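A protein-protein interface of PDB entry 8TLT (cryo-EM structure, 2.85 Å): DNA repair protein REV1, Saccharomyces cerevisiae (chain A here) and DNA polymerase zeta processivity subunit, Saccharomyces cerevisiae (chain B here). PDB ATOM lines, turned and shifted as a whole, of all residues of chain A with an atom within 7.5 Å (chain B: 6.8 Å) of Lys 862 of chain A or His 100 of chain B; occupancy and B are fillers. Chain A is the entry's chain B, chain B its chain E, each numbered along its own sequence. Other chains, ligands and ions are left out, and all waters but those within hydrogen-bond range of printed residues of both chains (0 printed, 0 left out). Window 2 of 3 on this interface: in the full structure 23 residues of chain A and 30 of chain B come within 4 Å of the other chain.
N of Lys 862 of chain A is in hydrogen-bond range of SD of Met 866 of chain A, 2.8 Å away.
Lys 862 of chain A touches His 100 of chain B (CB to O, 3.99 Å). Asn 863 of chain A touches His 71 of chain B (ND2 to NE2, 3.9 Å). Thr 70 of chain B touches Phe 865 of chain A (O to CZ, 3.3 Å). His 71 of chain B touches Phe 865 of chain A. CE of Met 866 of chain A touches O of Thr 70 of chain B, at 3.7 Å. His 100 of chain B touches Met 866 of chain A (CD2 to CE, 3.8 Å). His 100 of chain B touches Asn 869 of chain A. Ser 870 of chain A touches Leu 98 of chain B. NE2 of Gln 99 of chain B touches CB of Ser 870 of chain A (3.8 Å). Phe 95 of chain B touches Ile 871 of chain A.
Of the printed residues of chain B, Lys 862 of chain A touches His 100 (3.99 Å). Of the printed residues of chain A, His 100 of chain B touches Lys 862, Met 866 and Asn 869. Of the printed residues of chain B, Ile 871 of chain A touches Phe 95 (3.8 Å). Of the printed residues of chain A, Thr 70 of chain B touches Asn 863 (3.4 Å), Phe 865 (3.3 Å) and Met 866 (3.7 Å). Printed residues of chain B within 4 Å of Asn 863 of chain A: Thr 70 and His 71. His 864 of chain A touches none of the printed residues of chain B. The nearest printed residue of chain A that does not touch His 100 of chain B is Ser 870 of chain A (4.8 Å). The nearest printed residue of chain B that does not touch Asn 869 of chain A is Gln 99 of chain B (4.4 Å).
Hydrophobic or aromatic side chains of chain A within 4 Å of the printed part of chain B: Phe 865, Met 866 and Ile 871. Among the printed residues, 11 pairs touch across the chains. Among the printed residues, no Asp or Glu carboxylate lies within 4 Å of a Lys or Arg side-chain nitrogen of the other chain.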
ATOM      1  N   LYS A 862      -5.554  11.672  19.999  1.00  0.00           N
ATOM      2  CA  LYS A 862      -5.191  11.444  21.392  1.00  0.00           C
ATOM      3  C   LYS A 862      -5.246  12.740  22.192  1.00  0.00           C
ATOM      4  O   LYS A 862      -4.540  12.895  23.189  1.00  0.00           O
ATOM      5  CB  LYS A 862      -3.795  10.824  21.489  1.00  0.00           C
ATOM      6  N   ASN A 863      -6.087  13.668  21.750  1.00  0.00           N
ATOM      7  CA  ASN A 863      -6.276  14.942  22.435  1.00  0.00           C
ATOM      8  C   ASN A 863      -7.616  15.524  21.998  1.00  0.00           C
ATOM      9  O   ASN A 863      -8.412  14.858  21.329  1.00  0.00           O
ATOM     10  CB  ASN A 863      -5.111  15.895  22.152  1.00  0.00           C
ATOM     11  CG  ASN A 863      -4.142  15.990  23.314  1.00  0.00           C
ATOM     12  OD1 ASN A 863      -4.538  15.906  24.477  1.00  0.00           O
ATOM     13  ND2 ASN A 863      -2.863  16.167  23.006  1.00  0.00           N
ATOM     14  N   HIS A 864      -7.866  16.776  22.381  1.00  0.00           N
ATOM     15  CA  HIS A 864      -9.150  17.411  22.114  1.00  0.00           C
ATOM     16  C   HIS A 864      -9.188  18.149  20.784  1.00  0.00           C
ATOM     17  O   HIS A 864     -10.259  18.250  20.174  1.00  0.00           O
ATOM     18  CB  HIS A 864      -9.500  18.384  23.243  1.00  0.00           C
ATOM     19  N   PHE A 865      -8.052  18.667  20.317  1.00  0.00           N
ATOM     20  CA  PHE A 865      -8.028  19.427  19.074  1.00  0.00           C
ATOM     21  C   PHE A 865      -8.127  18.551  17.832  1.00  0.00           C
ATOM     22  O   PHE A 865      -8.346  19.081  16.738  1.00  0.00           O
ATOM     23  CB  PHE A 865      -6.759  20.282  19.002  1.00  0.00           C
ATOM     24  CG  PHE A 865      -5.486  19.489  19.061  1.00  0.00           C
ATOM     25  CD1 PHE A 865      -4.888  19.022  17.903  1.00  0.00           C
ATOM     26  CD2 PHE A 865      -4.879  19.217  20.274  1.00  0.00           C
ATOM     27  CE1 PHE A 865      -3.720  18.296  17.955  1.00  0.00           C
ATOM     28  CE2 PHE A 865      -3.710  18.491  20.328  1.00  0.00           C
ATOM     29  CZ  PHE A 865      -3.131  18.032  19.167  1.00  0.00           C
ATOM     30  N   MET A 866      -7.968  17.237  17.968  1.00  0.00           N
ATOM     31  CA  MET A 866      -8.058  16.350  16.817  1.00  0.00           C
ATOM     32  C   MET A 866      -9.487  16.285  16.296  1.00  0.00           C
ATOM     33  O   MET A 866     -10.447  16.245  17.070  1.00  0.00           O
ATOM     34  CB  MET A 866      -7.573  14.949  17.185  1.00  0.00           C
ATOM     35  CG  MET A 866      -6.306  14.924  18.016  1.00  0.00           C
ATOM     36  SD  MET A 866      -5.365  13.404  17.788  1.00  0.00           S
ATOM     37  CE  MET A 866      -3.693  14.027  17.877  1.00  0.00           C
ATOM     38  N   GLN A 868     -10.478  13.725  14.398  1.00  0.00           N
ATOM     39  CA  GLN A 868     -10.766  12.306  14.226  1.00  0.00           C
ATOM     40  C   GLN A 868      -9.796  11.529  15.114  1.00  0.00           C
ATOM     41  O   GLN A 868      -9.187  12.098  16.026  1.00  0.00           O
ATOM     42  CB  GLN A 868     -10.669  11.911  12.744  1.00  0.00           C
ATOM     43  N   ASN A 869      -9.666  10.225  14.860  1.00  0.00           N
ATOM     44  CA  ASN A 869      -8.626   9.449  15.527  1.00  0.00           C
ATOM     45  C   ASN A 869      -7.232   9.966  15.197  1.00  0.00           C
ATOM     46  O   ASN A 869      -6.284   9.684  15.937  1.00  0.00           O
ATOM     47  CB  ASN A 869      -8.741   7.973  15.145  1.00  0.00           C
ATOM     48  N   SER A 870      -7.090  10.707  14.103  1.00  0.00           N
ATOM     49  CA  SER A 870      -5.859  11.382  13.725  1.00  0.00           C
ATOM     50  C   SER A 870      -6.010  12.882  13.955  1.00  0.00           C
ATOM     51  O   SER A 870      -7.049  13.367  14.408  1.00  0.00           O
ATOM     52  CB  SER A 870      -5.507  11.079  12.267  1.00  0.00           C
ATOM     53  N   ILE A 871      -4.948  13.624  13.635  1.00  0.00           N
ATOM     54  CA  ILE A 871      -4.961  15.068  13.847  1.00  0.00           C
ATOM     55  C   ILE A 871      -5.967  15.742  12.920  1.00  0.00           C
ATOM     56  O   ILE A 871      -6.706  16.642  13.335  1.00  0.00           O
ATOM     57  CB  ILE A 871      -3.543  15.644  13.672  1.00  0.00           C
ATOM     58  CG1 ILE A 871      -3.594  17.161  13.476  1.00  0.00           C
ATOM     59  CG2 ILE A 871      -2.832  14.969  12.512  1.00  0.00           C
ATOM     60  N   VAL B   5       5.583   2.302  17.125  1.00  0.00           N
ATOM     61  CA  VAL B   5       5.321   3.376  16.170  1.00  0.00           C
ATOM     62  C   VAL B   5       6.401   4.444  16.257  1.00  0.00           C
ATOM     63  O   VAL B   5       6.885   4.944  15.233  1.00  0.00           O
ATOM     64  CB  VAL B   5       3.915   3.961  16.405  1.00  0.00           C
ATOM     65  CG1 VAL B   5       3.852   5.410  15.961  1.00  0.00           C
ATOM     66  CG2 VAL B   5       2.874   3.133  15.674  1.00  0.00           C
ATOM     67  N   GLU B   6       6.801   4.810  17.477  1.00  0.00           N
ATOM     68  CA  GLU B   6       7.825   5.838  17.638  1.00  0.00           C
ATOM     69  C   GLU B   6       9.163   5.381  17.070  1.00  0.00           C
ATOM     70  O   GLU B   6       9.886   6.177  16.464  1.00  0.00           O
ATOM     71  CB  GLU B   6       7.967   6.222  19.111  1.00  0.00           C
ATOM     72  CG  GLU B   6       6.752   6.932  19.701  1.00  0.00           C
ATOM     73  CD  GLU B   6       6.362   8.187  18.945  1.00  0.00           C
ATOM     74  OE1 GLU B   6       5.561   8.089  17.993  1.00  0.00           O
ATOM     75  OE2 GLU B   6       6.847   9.277  19.311  1.00  0.00           O
ATOM     76  N   LEU B   9       8.920   5.606  13.265  1.00  0.00           N
ATOM     77  CA  LEU B   9       8.967   7.008  12.871  1.00  0.00           C
ATOM     78  C   LEU B   9      10.376   7.568  13.001  1.00  0.00           C
ATOM     79  O   LEU B   9      10.825   8.341  12.148  1.00  0.00           O
ATOM     80  CB  LEU B   9       7.985   7.821  13.710  1.00  0.00           C
ATOM     81  CG  LEU B   9       6.590   7.990  13.112  1.00  0.00           C
ATOM     82  CD1 LEU B   9       5.561   8.174  14.209  1.00  0.00           C
ATOM     83  CD2 LEU B   9       6.559   9.160  12.146  1.00  0.00           C
ATOM     84  N   LEU B  69       4.803  15.334  18.312  1.00  0.00           N
ATOM     85  CA  LEU B  69       4.164  14.914  17.069  1.00  0.00           C
ATOM     86  C   LEU B  69       2.646  14.962  17.147  1.00  0.00           C
ATOM     87  O   LEU B  69       1.987  15.016  16.105  1.00  0.00           O
ATOM     88  CB  LEU B  69       4.617  13.503  16.695  1.00  0.00           C
ATOM     89  CG  LEU B  69       4.446  13.100  15.230  1.00  0.00           C
ATOM     90  CD1 LEU B  69       5.475  13.794  14.359  1.00  0.00           C
ATOM     91  CD2 LEU B  69       4.549  11.595  15.081  1.00  0.00           C
ATOM     92  N   THR B  70       2.079  14.938  18.354  1.00  0.00           N
ATOM     93  CA  THR B  70       0.629  15.011  18.489  1.00  0.00           C
ATOM     94  C   THR B  70       0.095  16.340  17.965  1.00  0.00           C
ATOM     95  O   THR B  70      -0.936  16.379  17.283  1.00  0.00           O
ATOM     96  CB  THR B  70       0.234  14.797  19.952  1.00  0.00           C
ATOM     97  OG1 THR B  70       0.215  13.392  20.237  1.00  0.00           O
ATOM     98  CG2 THR B  70      -1.138  15.374  20.237  1.00  0.00           C
ATOM     99  N   HIS B  71       0.794  17.436  18.254  1.00  0.00           N
ATOM    100  CA  HIS B  71       0.404  18.753  17.770  1.00  0.00           C
ATOM    101  C   HIS B  71       1.015  19.100  16.419  1.00  0.00           C
ATOM    102  O   HIS B  71       0.664  20.137  15.850  1.00  0.00           O
ATOM    103  CB  HIS B  71       0.797  19.832  18.783  1.00  0.00           C
ATOM    104  CG  HIS B  71       0.178  19.653  20.133  1.00  0.00           C
ATOM    105  ND1 HIS B  71      -0.866  20.433  20.581  1.00  0.00           N
ATOM    106  CD2 HIS B  71       0.460  18.790  21.137  1.00  0.00           C
ATOM    107  CE1 HIS B  71      -1.202  20.056  21.801  1.00  0.00           C
ATOM    108  NE2 HIS B  71      -0.414  19.059  22.161  1.00  0.00           N
ATOM    109  N   VAL B  72       1.913  18.271  15.897  1.00  0.00           N
ATOM    110  CA  VAL B  72       2.610  18.546  14.647  1.00  0.00           C
ATOM    111  C   VAL B  72       1.919  17.773  13.535  1.00  0.00           C
ATOM    112  O   VAL B  72       1.837  16.540  13.582  1.00  0.00           O
ATOM    113  CB  VAL B  72       4.097  18.168  14.739  1.00  0.00           C
ATOM    114  CG1 VAL B  72       4.700  18.019  13.354  1.00  0.00           C
ATOM    115  CG2 VAL B  72       4.852  19.199  15.546  1.00  0.00           C
ATOM    116  N   PHE B  95       2.382  14.837   8.153  1.00  0.00           N
ATOM    117  CA  PHE B  95       1.963  13.931   9.212  1.00  0.00           C
ATOM    118  C   PHE B  95       0.484  14.060   9.542  1.00  0.00           C
ATOM    119  O   PHE B  95       0.032  13.498  10.543  1.00  0.00           O
ATOM    120  CB  PHE B  95       2.801  14.159  10.470  1.00  0.00           C
ATOM    121  CG  PHE B  95       4.222  13.706  10.339  1.00  0.00           C
ATOM    122  CD1 PHE B  95       4.517  12.371  10.135  1.00  0.00           C
ATOM    123  CD2 PHE B  95       5.263  14.610  10.427  1.00  0.00           C
ATOM    124  CE1 PHE B  95       5.825  11.947  10.016  1.00  0.00           C
ATOM    125  CE2 PHE B  95       6.572  14.191  10.309  1.00  0.00           C
ATOM    126  CZ  PHE B  95       6.852  12.859  10.103  1.00  0.00           C
ATOM    127  N   LEU B  98      -2.444  10.963  10.399  1.00  0.00           N
ATOM    128  CA  LEU B  98      -1.627   9.907  10.982  1.00  0.00           C
ATOM    129  C   LEU B  98      -2.294   9.434  12.266  1.00  0.00           C
ATOM    130  O   LEU B  98      -2.528  10.236  13.177  1.00  0.00           O
ATOM    131  CB  LEU B  98      -0.209  10.402  11.261  1.00  0.00           C
ATOM    132  CG  LEU B  98       0.673   9.544  12.170  1.00  0.00           C
ATOM    133  CD1 LEU B  98       0.907   8.185  11.556  1.00  0.00           C
ATOM    134  CD2 LEU B  98       1.997  10.231  12.447  1.00  0.00           C
ATOM    135  N   GLN B  99      -2.603   8.142  12.334  1.00  0.00           N
ATOM    136  CA  GLN B  99      -3.309   7.599  13.487  1.00  0.00           C
ATOM    137  C   GLN B  99      -2.439   7.678  14.735  1.00  0.00           C
ATOM    138  O   GLN B  99      -1.270   7.283  14.719  1.00  0.00           O
ATOM    139  CB  GLN B  99      -3.724   6.154  13.221  1.00  0.00           C
ATOM    140  CG  GLN B  99      -5.209   5.973  12.959  1.00  0.00           C
ATOM    141  CD  GLN B  99      -5.591   6.287  11.529  1.00  0.00           C
ATOM    142  OE1 GLN B  99      -5.329   5.502  10.618  1.00  0.00           O
ATOM    143  NE2 GLN B  99      -6.218   7.439  11.322  1.00  0.00           N
ATOM    144  N   HIS B 100      -3.016   8.190  15.817  1.00  0.00           N
ATOM    145  CA  HIS B 100      -2.344   8.311  17.108  1.00  0.00           C
ATOM    146  C   HIS B 100      -3.105   7.425  18.089  1.00  0.00           C
ATOM    147  O   HIS B 100      -4.004   7.890  18.794  1.00  0.00           O
ATOM    148  CB  HIS B 100      -2.300   9.765  17.571  1.00  0.00           C
ATOM    149  CG  HIS B 100      -1.166  10.550  16.988  1.00  0.00           C
ATOM    150  ND1 HIS B 100       0.154  10.194  17.161  1.00  0.00           N
ATOM    151  CD2 HIS B 100      -1.156  11.671  16.230  1.00  0.00           C
ATOM    152  CE1 HIS B 100       0.928  11.061  16.536  1.00  0.00           C
ATOM    153  NE2 HIS B 100       0.158  11.967  15.962  1.00  0.00           N
ATOM    154  N   VAL B 101      -2.743   6.146  18.133  1.00  0.00           N
ATOM    155  CA  VAL B 101      -3.416   5.158  18.966  1.00  0.00           C
ATOM    156  C   VAL B 101      -2.399   4.561  19.926  1.00  0.00           C
ATOM    157  O   VAL B 101      -1.323   4.119  19.505  1.00  0.00           O
ATOM    158  CB  VAL B 101      -4.081   4.056  18.119  1.00  0.00           C
ATOM    159  CG1 VAL B 101      -5.438   4.522  17.618  1.00  0.00           C
ATOM    160  CG2 VAL B 101      -3.185   3.664  16.953  1.00  0.00           C
ATOM    161  N   ASP B 102      -2.737   4.554  21.213  1.00  0.00           N
ATOM    162  CA  ASP B 102      -1.876   3.992  22.243  1.00  0.00           C
ATOM    163  C   ASP B 102      -2.161   2.522  22.517  1.00  0.00           C
ATOM    164  O   ASP B 102      -1.464   1.914  23.335  1.00  0.00           O
ATOM    165  CB  ASP B 102      -2.017   4.792  23.542  1.00  0.00           C
ATOM    166  N   LYS B 103      -3.159   1.941  21.859  1.00  0.00           N
ATOM    167  CA  LYS B 103      -3.511   0.542  22.074  1.00  0.00           C
ATOM    168  C   LYS B 103      -2.486  -0.388  21.435  1.00  0.00           C
ATOM    169  O   LYS B 103      -1.452  -0.690  22.031  1.00  0.00           O
ATOM    170  CB  LYS B 103      -4.905   0.249  21.516  1.00  0.00           C
ATOM    171  N   PRO B 209      -0.904   1.773  10.975  1.00  0.00           N
ATOM    172  CA  PRO B 209      -0.892   2.875  11.947  1.00  0.00           C
ATOM    173  C   PRO B 209      -0.240   4.135  11.403  1.00  0.00           C
ATOM    174  O   PRO B 209      -0.463   5.229  11.930  1.00  0.00           O
ATOM    175  CB  PRO B 209      -0.097   2.294  13.122  1.00  0.00           C
